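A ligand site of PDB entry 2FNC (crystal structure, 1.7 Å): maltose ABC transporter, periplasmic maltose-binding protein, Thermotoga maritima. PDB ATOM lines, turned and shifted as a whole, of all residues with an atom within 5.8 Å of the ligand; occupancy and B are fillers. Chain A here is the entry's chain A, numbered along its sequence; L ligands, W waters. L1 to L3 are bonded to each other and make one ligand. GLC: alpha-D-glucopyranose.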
ATOM      1  N   SER A   8      33.278 -17.542  20.069  1.00  0.00           N
ATOM      2  CA  SER A   8      32.686 -16.326  20.647  1.00  0.00           C
ATOM      3  C   SER A   8      33.396 -15.934  21.918  1.00  0.00           C
ATOM      4  O   SER A   8      34.220 -16.697  22.430  1.00  0.00           O
ATOM      5  CB  SER A   8      31.196 -16.498  20.900  1.00  0.00           C
ATOM      6  OG  SER A   8      30.942 -17.163  22.105  1.00  0.00           O
ATOM      7  N   GLU A   9      33.062 -14.750  22.429  1.00  0.00           N
ATOM      8  CA  GLU A   9      33.639 -14.255  23.666  1.00  0.00           C
ATOM      9  C   GLU A   9      33.370 -15.169  24.853  1.00  0.00           C
ATOM     10  O   GLU A   9      34.133 -15.172  25.819  1.00  0.00           O
ATOM     11  CB  GLU A   9      33.182 -12.822  23.940  1.00  0.00           C
ATOM     12  CG  GLU A   9      31.742 -12.628  24.350  1.00  0.00           C
ATOM     13  CD  GLU A   9      30.745 -12.853  23.265  1.00  0.00           C
ATOM     14  OE1 GLU A   9      31.073 -12.730  22.051  1.00  0.00           O
ATOM     15  OE2 GLU A   9      29.602 -13.179  23.637  1.00  0.00           O
ATOM     16  N   LYS A  10      32.294 -15.957  24.815  1.00  0.00           N
ATOM     17  CA  LYS A  10      31.936 -16.757  25.964  1.00  0.00           C
ATOM     18  C   LYS A  10      32.923 -17.881  26.260  1.00  0.00           C
ATOM     19  O   LYS A  10      33.103 -18.266  27.396  1.00  0.00           O
ATOM     20  CB  LYS A  10      30.518 -17.320  25.805  1.00  0.00           C
ATOM     21  CG  LYS A  10      29.403 -16.269  25.597  1.00  0.00           C
ATOM     22  CD  LYS A  10      29.130 -15.453  26.846  1.00  0.00           C
ATOM     23  CE  LYS A  10      28.092 -14.370  26.617  1.00  0.00           C
ATOM     24  NZ  LYS A  10      27.891 -13.574  27.860  1.00  0.00           N
ATOM     25  N   GLN A  11      33.576 -18.430  25.217  1.00  0.00           N
ATOM     26  CA  GLN A  11      34.492 -19.548  25.352  1.00  0.00           C
ATOM     27  C   GLN A  11      35.991 -19.164  25.298  1.00  0.00           C
ATOM     28  O   GLN A  11      36.844 -20.002  25.514  1.00  0.00           O
ATOM     29  CB  GLN A  11      34.254 -20.594  24.248  1.00  0.00           C
ATOM     30  CG  GLN A  11      32.803 -21.057  24.142  1.00  0.00           C
ATOM     31  CD  GLN A  11      31.973 -20.294  23.143  1.00  0.00           C
ATOM     32  OE1 GLN A  11      32.368 -19.197  22.685  1.00  0.00           O
ATOM     33  NE2 GLN A  11      30.826 -20.838  22.799  1.00  0.00           N
ATOM     34  N   PHE A  37      30.063 -14.001  17.462  1.00  0.00           N
ATOM     35  CA  PHE A  37      29.337 -15.238  17.061  1.00  0.00           C
ATOM     36  C   PHE A  37      28.612 -15.107  15.715  1.00  0.00           C
ATOM     37  O   PHE A  37      28.665 -15.997  14.872  1.00  0.00           O
ATOM     38  CB  PHE A  37      28.368 -15.671  18.180  1.00  0.00           C
ATOM     39  CG  PHE A  37      27.504 -16.822  17.769  1.00  0.00           C
ATOM     40  CD1 PHE A  37      27.939 -18.128  17.957  1.00  0.00           C
ATOM     41  CD2 PHE A  37      26.279 -16.601  17.160  1.00  0.00           C
ATOM     42  CE1 PHE A  37      27.135 -19.225  17.541  1.00  0.00           C
ATOM     43  CE2 PHE A  37      25.478 -17.683  16.706  1.00  0.00           C
ATOM     44  CZ  PHE A  37      25.919 -18.986  16.921  1.00  0.00           C
ATOM     45  N   LYS A  41      30.386 -18.101  11.057  1.00  0.00           N
ATOM     46  CA  LYS A  41      30.106 -18.942   9.886  1.00  0.00           C
ATOM     47  C   LYS A  41      30.451 -18.170   8.576  1.00  0.00           C
ATOM     48  O   LYS A  41      31.063 -18.746   7.676  1.00  0.00           O
ATOM     49  CB  LYS A  41      28.643 -19.448   9.839  1.00  0.00           C
ATOM     50  CG  LYS A  41      28.368 -20.318   8.597  1.00  0.00           C
ATOM     51  CD  LYS A  41      27.105 -21.183   8.623  1.00  0.00           C
ATOM     52  CE  LYS A  41      25.811 -20.364   8.627  1.00  0.00           C
ATOM     53  NZ  LYS A  41      25.441 -19.822   7.301  1.00  0.00           N
ATOM     54  N   ALA A  60      27.244 -23.323  16.578  1.00  0.00           N
ATOM     55  CA  ALA A  60      25.917 -23.953  16.640  1.00  0.00           C
ATOM     56  C   ALA A  60      25.749 -25.036  15.598  1.00  0.00           C
ATOM     57  O   ALA A  60      26.268 -24.959  14.495  1.00  0.00           O
ATOM     58  CB  ALA A  60      24.820 -22.926  16.460  1.00  0.00           C
ATOM     59  N   HIS A  61      24.966 -26.036  15.952  1.00  0.00           N
ATOM     60  CA  HIS A  61      24.848 -27.222  15.116  1.00  0.00           C
ATOM     61  C   HIS A  61      24.064 -26.977  13.827  1.00  0.00           C
ATOM     62  O   HIS A  61      24.199 -27.777  12.890  1.00  0.00           O
ATOM     63  CB  HIS A  61      24.129 -28.330  15.921  1.00  0.00           C
ATOM     64  CG  HIS A  61      22.657 -28.133  16.024  1.00  0.00           C
ATOM     65  ND1 HIS A  61      22.075 -27.425  17.046  1.00  0.00           N
ATOM     66  CD2 HIS A  61      21.638 -28.590  15.249  1.00  0.00           C
ATOM     67  CE1 HIS A  61      20.768 -27.424  16.890  1.00  0.00           C
ATOM     68  NE2 HIS A  61      20.470 -28.125  15.800  1.00  0.00           N
ATOM     69  N   ASP A  62      23.276 -25.899  13.757  1.00  0.00           N
ATOM     70  CA  ASP A  62      22.507 -25.599  12.539  1.00  0.00           C
ATOM     71  C   ASP A  62      23.417 -25.364  11.325  1.00  0.00           C
ATOM     72  O   ASP A  62      23.006 -25.546  10.189  1.00  0.00           O
ATOM     73  CB  ASP A  62      21.479 -24.478  12.711  1.00  0.00           C
ATOM     74  CG  ASP A  62      22.093 -23.137  13.058  1.00  0.00           C
ATOM     75  OD1 ASP A  62      22.650 -23.042  14.180  1.00  0.00           O
ATOM     76  OD2 ASP A  62      21.990 -22.192  12.231  1.00  0.00           O
ATOM     77  N   TRP A  63      24.660 -24.963  11.556  1.00  0.00           N
ATOM     78  CA  TRP A  63      25.631 -24.788  10.489  1.00  0.00           C
ATOM     79  C   TRP A  63      26.104 -26.054   9.790  1.00  0.00           C
ATOM     80  O   TRP A  63      26.728 -25.982   8.737  1.00  0.00           O
ATOM     81  CB  TRP A  63      26.900 -24.150  11.043  1.00  0.00           C
ATOM     82  CG  TRP A  63      26.696 -22.929  11.885  1.00  0.00           C
ATOM     83  CD1 TRP A  63      25.576 -22.184  12.043  1.00  0.00           C
ATOM     84  CD2 TRP A  63      27.723 -22.295  12.667  1.00  0.00           C
ATOM     85  NE1 TRP A  63      25.840 -21.127  12.915  1.00  0.00           N
ATOM     86  CE2 TRP A  63      27.143 -21.177  13.304  1.00  0.00           C
ATOM     87  CE3 TRP A  63      29.083 -22.547  12.879  1.00  0.00           C
ATOM     88  CZ2 TRP A  63      27.874 -20.316  14.121  1.00  0.00           C
ATOM     89  CZ3 TRP A  63      29.796 -21.696  13.737  1.00  0.00           C
ATOM     90  CH2 TRP A  63      29.186 -20.592  14.332  1.00  0.00           C
ATOM     91  N   GLU A 107      21.310 -26.115  24.691  1.00  0.00           N
ATOM     92  CA  GLU A 107      20.758 -24.857  25.167  1.00  0.00           C
ATOM     93  C   GLU A 107      19.402 -24.554  24.555  1.00  0.00           C
ATOM     94  O   GLU A 107      19.054 -25.026  23.485  1.00  0.00           O
ATOM     95  CB  GLU A 107      21.719 -23.683  24.870  1.00  0.00           C
ATOM     96  CG  GLU A 107      21.906 -23.494  23.358  1.00  0.00           C
ATOM     97  CD  GLU A 107      23.083 -22.623  22.957  1.00  0.00           C
ATOM     98  OE1 GLU A 107      23.936 -22.320  23.815  1.00  0.00           O
ATOM     99  OE2 GLU A 107      23.161 -22.279  21.763  1.00  0.00           O
ATOM    100  N   ASP A 149      15.210  -9.556  21.772  1.00  0.00           N
ATOM    101  CA  ASP A 149      15.682  -9.322  20.405  1.00  0.00           C
ATOM    102  C   ASP A 149      14.571  -9.751  19.428  1.00  0.00           C
ATOM    103  O   ASP A 149      14.681 -10.803  18.774  1.00  0.00           O
ATOM    104  CB  ASP A 149      16.968 -10.130  20.153  1.00  0.00           C
ATOM    105  CG  ASP A 149      17.715  -9.752  18.884  1.00  0.00           C
ATOM    106  OD1 ASP A 149      17.387  -8.700  18.267  1.00  0.00           O
ATOM    107  OD2 ASP A 149      18.662 -10.511  18.496  1.00  0.00           O
ATOM    108  N   ASN A 152      14.792 -10.886  15.578  1.00  0.00           N
ATOM    109  CA  ASN A 152      15.622 -12.045  15.336  1.00  0.00           C
ATOM    110  C   ASN A 152      14.744 -13.318  15.394  1.00  0.00           C
ATOM    111  O   ASN A 152      14.147 -13.611  16.424  1.00  0.00           O
ATOM    112  CB  ASN A 152      16.718 -12.064  16.421  1.00  0.00           C
ATOM    113  CG  ASN A 152      17.721 -13.167  16.222  1.00  0.00           C
ATOM    114  OD1 ASN A 152      17.429 -14.179  15.562  1.00  0.00           O
ATOM    115  ND2 ASN A 152      18.895 -13.036  16.858  1.00  0.00           N
ATOM    116  N   PHE A 153      14.709 -14.089  14.315  1.00  0.00           N
ATOM    117  CA  PHE A 153      13.813 -15.268  14.285  1.00  0.00           C
ATOM    118  C   PHE A 153      14.173 -16.277  15.378  1.00  0.00           C
ATOM    119  O   PHE A 153      13.318 -16.994  15.918  1.00  0.00           O
ATOM    120  CB  PHE A 153      13.788 -15.903  12.889  1.00  0.00           C
ATOM    121  CG  PHE A 153      12.963 -17.166  12.796  1.00  0.00           C
ATOM    122  CD1 PHE A 153      11.653 -17.193  13.284  1.00  0.00           C
ATOM    123  CD2 PHE A 153      13.514 -18.346  12.281  1.00  0.00           C
ATOM    124  CE1 PHE A 153      10.908 -18.370  13.251  1.00  0.00           C
ATOM    125  CE2 PHE A 153      12.763 -19.526  12.221  1.00  0.00           C
ATOM    126  CZ  PHE A 153      11.465 -19.534  12.711  1.00  0.00           C
ATOM    127  N   TYR A 154      15.459 -16.377  15.704  1.00  0.00           N
ATOM    128  CA  TYR A 154      15.850 -17.295  16.722  1.00  0.00           C
ATOM    129  C   TYR A 154      15.085 -17.057  18.044  1.00  0.00           C
ATOM    130  O   TYR A 154      14.601 -17.999  18.662  1.00  0.00           O
ATOM    131  CB  TYR A 154      17.369 -17.238  16.964  1.00  0.00           C
ATOM    132  CG  TYR A 154      17.819 -18.195  18.054  1.00  0.00           C
ATOM    133  CD1 TYR A 154      18.059 -19.528  17.777  1.00  0.00           C
ATOM    134  CD2 TYR A 154      17.997 -17.748  19.345  1.00  0.00           C
ATOM    135  CE1 TYR A 154      18.455 -20.423  18.790  1.00  0.00           C
ATOM    136  CE2 TYR A 154      18.400 -18.597  20.337  1.00  0.00           C
ATOM    137  CZ  TYR A 154      18.643 -19.928  20.074  1.00  0.00           C
ATOM    138  OH  TYR A 154      19.026 -20.760  21.097  1.00  0.00           O
ATOM    139  N   PHE A 155      14.991 -15.793  18.443  1.00  0.00           N
ATOM    140  CA  PHE A 155      14.427 -15.409  19.719  1.00  0.00           C
ATOM    141  C   PHE A 155      12.893 -15.354  19.707  1.00  0.00           C
ATOM    142  O   PHE A 155      12.261 -15.556  20.755  1.00  0.00           O
ATOM    143  CB  PHE A 155      15.055 -14.092  20.176  1.00  0.00           C
ATOM    144  CG  PHE A 155      16.486 -14.249  20.616  1.00  0.00           C
ATOM    145  CD1 PHE A 155      16.807 -14.929  21.787  1.00  0.00           C
ATOM    146  CD2 PHE A 155      17.513 -13.713  19.836  1.00  0.00           C
ATOM    147  CE1 PHE A 155      18.128 -15.077  22.170  1.00  0.00           C
ATOM    148  CE2 PHE A 155      18.830 -13.874  20.213  1.00  0.00           C
ATOM    149  CZ  PHE A 155      19.141 -14.551  21.364  1.00  0.00           C
ATOM    150  N   TYR A 209      19.360  -7.369  20.749  1.00  0.00           N
ATOM    151  CA  TYR A 209      20.037  -8.191  21.715  1.00  0.00           C
ATOM    152  C   TYR A 209      20.919  -7.375  22.651  1.00  0.00           C
ATOM    153  O   TYR A 209      20.867  -7.563  23.850  1.00  0.00           O
ATOM    154  CB  TYR A 209      20.917  -9.245  21.020  1.00  0.00           C
ATOM    155  CG  TYR A 209      21.470 -10.208  22.023  1.00  0.00           C
ATOM    156  CD1 TYR A 209      20.733 -11.314  22.431  1.00  0.00           C
ATOM    157  CD2 TYR A 209      22.701 -10.005  22.608  1.00  0.00           C
ATOM    158  CE1 TYR A 209      21.247 -12.187  23.394  1.00  0.00           C
ATOM    159  CE2 TYR A 209      23.201 -10.859  23.536  1.00  0.00           C
ATOM    160  CZ  TYR A 209      22.484 -11.956  23.946  1.00  0.00           C
ATOM    161  OH  TYR A 209      23.027 -12.783  24.912  1.00  0.00           O
ATOM    162  N   ASN A 226      16.302 -14.939  26.943  1.00  0.00           N
ATOM    163  CA  ASN A 226      17.692 -15.249  26.609  1.00  0.00           C
ATOM    164  C   ASN A 226      18.093 -16.673  27.089  1.00  0.00           C
ATOM    165  O   ASN A 226      17.344 -17.354  27.798  1.00  0.00           O
ATOM    166  CB  ASN A 226      18.618 -14.158  27.168  1.00  0.00           C
ATOM    167  CG  ASN A 226      19.897 -13.983  26.362  1.00  0.00           C
ATOM    168  OD1 ASN A 226      20.135 -14.677  25.354  1.00  0.00           O
ATOM    169  ND2 ASN A 226      20.742 -13.020  26.786  1.00  0.00           N
ATOM    170  N   TRP A 229      23.956 -18.969  27.965  1.00  0.00           N
ATOM    171  CA  TRP A 229      25.212 -18.289  27.650  1.00  0.00           C
ATOM    172  C   TRP A 229      25.371 -16.932  28.319  1.00  0.00           C
ATOM    173  O   TRP A 229      26.477 -16.390  28.314  1.00  0.00           O
ATOM    174  CB  TRP A 229      25.377 -18.121  26.145  1.00  0.00           C
ATOM    175  CG  TRP A 229      24.222 -17.436  25.509  1.00  0.00           C
ATOM    176  CD1 TRP A 229      24.019 -16.094  25.449  1.00  0.00           C
ATOM    177  CD2 TRP A 229      23.109 -18.052  24.854  1.00  0.00           C
ATOM    178  NE1 TRP A 229      22.837 -15.813  24.795  1.00  0.00           N
ATOM    179  CE2 TRP A 229      22.246 -16.999  24.438  1.00  0.00           C
ATOM    180  CE3 TRP A 229      22.740 -19.381  24.605  1.00  0.00           C
ATOM    181  CZ2 TRP A 229      21.040 -17.232  23.764  1.00  0.00           C
ATOM    182  CZ3 TRP A 229      21.514 -19.611  23.920  1.00  0.00           C
ATOM    183  CH2 TRP A 229      20.704 -18.549  23.522  1.00  0.00           C
ATOM    184  N   GLY A 260      19.343 -25.646  20.738  1.00  0.00           N
ATOM    185  CA  GLY A 260      20.656 -25.570  20.141  1.00  0.00           C
ATOM    186  C   GLY A 260      21.678 -26.459  20.779  1.00  0.00           C
ATOM    187  O   GLY A 260      21.661 -26.701  21.971  1.00  0.00           O
ATOM    188  N   GLN A 262      25.907 -26.614  20.947  1.00  0.00           N
ATOM    189  CA  GLN A 262      27.167 -25.934  20.689  1.00  0.00           C
ATOM    190  C   GLN A 262      28.272 -26.976  20.636  1.00  0.00           C
ATOM    191  O   GLN A 262      28.317 -27.953  21.451  1.00  0.00           O
ATOM    192  CB  GLN A 262      27.466 -24.920  21.806  1.00  0.00           C
ATOM    193  CG  GLN A 262      26.510 -23.744  21.840  1.00  0.00           C
ATOM    194  CD  GLN A 262      26.697 -22.777  20.722  1.00  0.00           C
ATOM    195  OE1 GLN A 262      27.813 -22.571  20.232  1.00  0.00           O
ATOM    196  NE2 GLN A 262      25.619 -22.180  20.291  1.00  0.00           N
ATOM    197  N   ARG A 299      26.431 -23.876  30.189  1.00  0.00           N
ATOM    198  CA  ARG A 299      25.298 -24.349  29.405  1.00  0.00           C
ATOM    199  C   ARG A 299      25.065 -25.808  29.769  1.00  0.00           C
ATOM    200  O   ARG A 299      25.923 -26.402  30.472  1.00  0.00           O
ATOM    201  CB  ARG A 299      25.595 -24.178  27.929  1.00  0.00           C
ATOM    202  CG  ARG A 299      26.090 -22.781  27.596  1.00  0.00           C
ATOM    203  CD  ARG A 299      26.290 -22.595  26.162  1.00  0.00           C
ATOM    204  NE  ARG A 299      27.222 -21.497  25.902  1.00  0.00           N
ATOM    205  CZ  ARG A 299      27.263 -20.757  24.813  1.00  0.00           C
ATOM    206  NH1 ARG A 299      26.336 -20.843  23.865  1.00  0.00           N
ATOM    207  NH2 ARG A 299      28.210 -19.818  24.708  1.00  0.00           N
ATOM    208  N   MET A 329      16.960 -27.050  16.270  1.00  0.00           N
ATOM    209  CA  MET A 329      17.080 -26.395  14.971  1.00  0.00           C
ATOM    210  C   MET A 329      17.439 -27.433  13.920  1.00  0.00           C
ATOM    211  O   MET A 329      18.275 -28.318  14.168  1.00  0.00           O
ATOM    212  CB  MET A 329      18.218 -25.340  14.964  1.00  0.00           C
ATOM    213  CG  MET A 329      18.001 -24.215  15.923  1.00  0.00           C
ATOM    214  SD  MET A 329      19.292 -22.939  15.813  1.00  0.00           S
ATOM    215  CE  MET A 329      20.545 -23.773  16.715  1.00  0.00           C
ATOM    216  N   TRP A 339      17.085 -17.690   8.254  1.00  0.00           N
ATOM    217  CA  TRP A 339      17.200 -16.704   9.326  1.00  0.00           C
ATOM    218  C   TRP A 339      16.992 -15.285   8.784  1.00  0.00           C
ATOM    219  O   TRP A 339      16.242 -14.515   9.377  1.00  0.00           O
ATOM    220  CB  TRP A 339      18.556 -16.795  10.022  1.00  0.00           C
ATOM    221  CG  TRP A 339      18.828 -18.179  10.604  1.00  0.00           C
ATOM    222  CD1 TRP A 339      19.743 -19.085  10.131  1.00  0.00           C
ATOM    223  CD2 TRP A 339      18.205 -18.798  11.745  1.00  0.00           C
ATOM    224  NE1 TRP A 339      19.722 -20.221  10.899  1.00  0.00           N
ATOM    225  CE2 TRP A 339      18.783 -20.085  11.871  1.00  0.00           C
ATOM    226  CE3 TRP A 339      17.196 -18.415  12.643  1.00  0.00           C
ATOM    227  CZ2 TRP A 339      18.411 -20.974  12.895  1.00  0.00           C
ATOM    228  CZ3 TRP A 339      16.818 -19.308  13.640  1.00  0.00           C
ATOM    229  CH2 TRP A 339      17.469 -20.560  13.783  1.00  0.00           C
HETATM  230  C1  GLC L   1      27.325 -15.544  22.540  1.00  0.00           C
HETATM  231  C2  GLC L   1      27.124 -17.049  22.611  1.00  0.00           C
HETATM  232  C3  GLC L   1      26.293 -17.566  21.432  1.00  0.00           C
HETATM  233  C4  GLC L   1      24.985 -16.786  21.407  1.00  0.00           C
HETATM  234  C5  GLC L   1      25.242 -15.293  21.259  1.00  0.00           C
HETATM  235  C6  GLC L   1      23.980 -14.419  21.301  1.00  0.00           C
HETATM  236  O1  GLC L   1      28.280 -15.284  21.531  1.00  0.00           O
HETATM  237  O2  GLC L   1      28.367 -17.697  22.634  1.00  0.00           O
HETATM  238  O3  GLC L   1      26.081 -18.982  21.590  1.00  0.00           O
HETATM  239  O4  GLC L   1      24.171 -17.207  20.293  1.00  0.00           O
HETATM  240  O5  GLC L   1      26.094 -14.825  22.324  1.00  0.00           O
HETATM  241  O6  GLC L   1      24.319 -13.112  20.794  1.00  0.00           O
HETATM  242  C1  GLC L   2      22.848 -17.567  20.613  1.00  0.00           C
HETATM  243  C2  GLC L   2      22.679 -19.060  20.261  1.00  0.00           C
HETATM  244  C3  GLC L   2      22.759 -19.195  18.753  1.00  0.00           C
HETATM  245  C4  GLC L   2      21.821 -18.253  18.011  1.00  0.00           C
HETATM  246  C5  GLC L   2      22.012 -16.804  18.479  1.00  0.00           C
HETATM  247  C6  GLC L   2      20.928 -15.900  17.911  1.00  0.00           C
HETATM  248  O2  GLC L   2      23.703 -19.880  20.884  1.00  0.00           O
HETATM  249  O3  GLC L   2      22.452 -20.563  18.372  1.00  0.00           O
HETATM  250  O4  GLC L   2      22.096 -18.345  16.623  1.00  0.00           O
HETATM  251  O5  GLC L   2      21.923 -16.766  19.899  1.00  0.00           O
HETATM  252  O6  GLC L   2      21.472 -14.586  17.752  1.00  0.00           O
HETATM  253  C1  GLC L   3      21.083 -18.977  15.846  1.00  0.00           C
HETATM  254  C2  GLC L   3      21.771 -19.904  14.834  1.00  0.00           C
HETATM  255  C3  GLC L   3      22.552 -19.067  13.801  1.00  0.00           C
HETATM  256  C4  GLC L   3      21.653 -18.010  13.160  1.00  0.00           C
HETATM  257  C5  GLC L   3      20.980 -17.180  14.246  1.00  0.00           C
HETATM  258  C6  GLC L   3      20.066 -16.121  13.651  1.00  0.00           C
HETATM  259  O2  GLC L   3      22.660 -20.803  15.546  1.00  0.00           O
HETATM  260  O3  GLC L   3      23.124 -19.928  12.792  1.00  0.00           O
HETATM  261  O4  GLC L   3      22.439 -17.144  12.312  1.00  0.00           O
HETATM  262  O5  GLC L   3      20.270 -18.030  15.156  1.00  0.00           O
HETATM  263  O6  GLC L   3      19.819 -15.071  14.604  1.00  0.00           O
HETATM  264  O   HOH W   1      28.889 -20.021  20.735  1.00  0.00           O
HETATM  265  O   HOH W   2      29.535 -12.928  20.191  1.00  0.00           O
HETATM  266  O   HOH W   3      21.004 -22.197  20.082  1.00  0.00           O
HETATM  267  O   HOH W   4      25.524 -17.974  12.551  1.00  0.00           O
HETATM  268  O   HOH W   5      23.555 -14.289  15.987  1.00  0.00           O
HETATM  269  O   HOH W   6      20.814 -12.687  13.746  1.00  0.00           O
HETATM  270  O   HOH W   7      22.145 -12.442  19.300  1.00  0.00           O
HETATM  271  O   HOH W   8      25.201 -13.214  17.944  1.00  0.00           O
HETATM  272  O   HOH W   9      26.946 -12.396  19.568  1.00  0.00           O
HETATM  273  O   HOH W  10      24.030 -15.392  13.565  1.00  0.00           O
HETATM  274  O   HOH W  11      23.105 -17.149   9.671  1.00  0.00           O
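Water W3 lies within hydrogen-bond range of OH of Tyr 154 (2.6 Å), OE2 of Glu 107 (2.7 Å) and O3 of GLC L2 (2.8 Å).
Water W2 lies within hydrogen-bond range of OE1 of Glu 9 (2.4 Å), N of Phe 37 (3.0 Å) and O1 of GLC L1 (3.0 Å).
Water W1 lies within hydrogen-bond range of OE1 of Gln 262 (2.8 Å), NE2 of Gln 11 (2.9 Å) and O2 of GLC L1 (3.0 Å).
Water W4 lies within hydrogen-bond range of O3 of GLC L3 (3.1 Å) and NE1 of Trp 63 (3.2 Å).
OD2 of Asp 62 lies within hydrogen-bond range of NE1 of Trp 339, at 3.3 Å.
OE2 of Glu 107 lies within hydrogen-bond range of NE2 of Gln 262 (2.9 Å).
The backbone carbonyl oxygen (O) of Gly 260 sits at hydrogen-bond distance from the backbone NH (N) of Glu 107 (2.8 Å).
The side-chain hydroxyl (OG) of Ser 8 is in hydrogen-bond range of the side-chain amide oxygen (OE1) of Gln 11 (2.6 Å).
The guanidinium group (NH2) of Arg 299 lies close to the side-chain amide nitrogen (NE2) of Gln 11 (3.4 Å).
The side-chain amino group of Lys 10 lies close to the backbone carbonyl oxygen of Trp 229 (3.2 Å).
The side-chain hydroxyl (OH) of Tyr 209 is in hydrogen-bond range of the indole nitrogen (NE1) of Trp 229, at 3.0 Å.
NE2 of His 61 is in hydrogen-bond range of O of Met 329, 2.7 Å away.
OD2 of Asp 62 sits at hydrogen-bond distance from O3 of GLC L3 (2.6 Å).
The side-chain carboxylate (OE2) of Glu 107 lies within hydrogen-bond range of an oxygen (O2) of GLC L2, at 2.6 Å.
The side-chain hydroxyl (OG) of Ser 8 is in hydrogen-bond range of an oxygen (O2) of GLC L1.
The side-chain amide oxygen (OD1) of Asn 152 is in hydrogen-bond range of an oxygen (O6) of GLC L3 (2.7 Å).
The guanidinium group (NH1) of Arg 299 is in hydrogen-bond range of an oxygen (O3) of GLC L1 (3.0 Å).
An oxygen (O3) of GLC L3 lies within hydrogen-bond range of the indole nitrogen of Trp 63 (3.0 Å).
The side-chain amide nitrogen (NE2) of Gln 262 sits at hydrogen-bond distance from an oxygen (O2) of GLC L2, at 3.1 Å.
The side-chain carboxylate (OE2) of Glu 9 lies within hydrogen-bond range of an oxygen (O1) of GLC L1 (3.3 Å).
Residues that only touch the ligand: Lys 10, Gln 11, Phe 37, Ala 60, Tyr 154, Phe 155, Tyr 209, Trp 229, Met 329 and Trp 339.
Hydrophobic or aromatic side chains within 4 Å of the ligand: Phe 37, Ala 60, Trp 63, Tyr 154, Phe 155, Tyr 209, Trp 229, Met 329 and Trp 339.
18 residues have an atom within 4 Å of the ligand: Ser 8, Glu 9, Lys 10, Gln 11, Phe 37, Ala 60, Asp 62, Trp 63, Glu 107, Asn 152, Tyr 154, Phe 155, Tyr 209, Trp 229, Gln 262, Arg 299, Met 329 and Trp 339.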
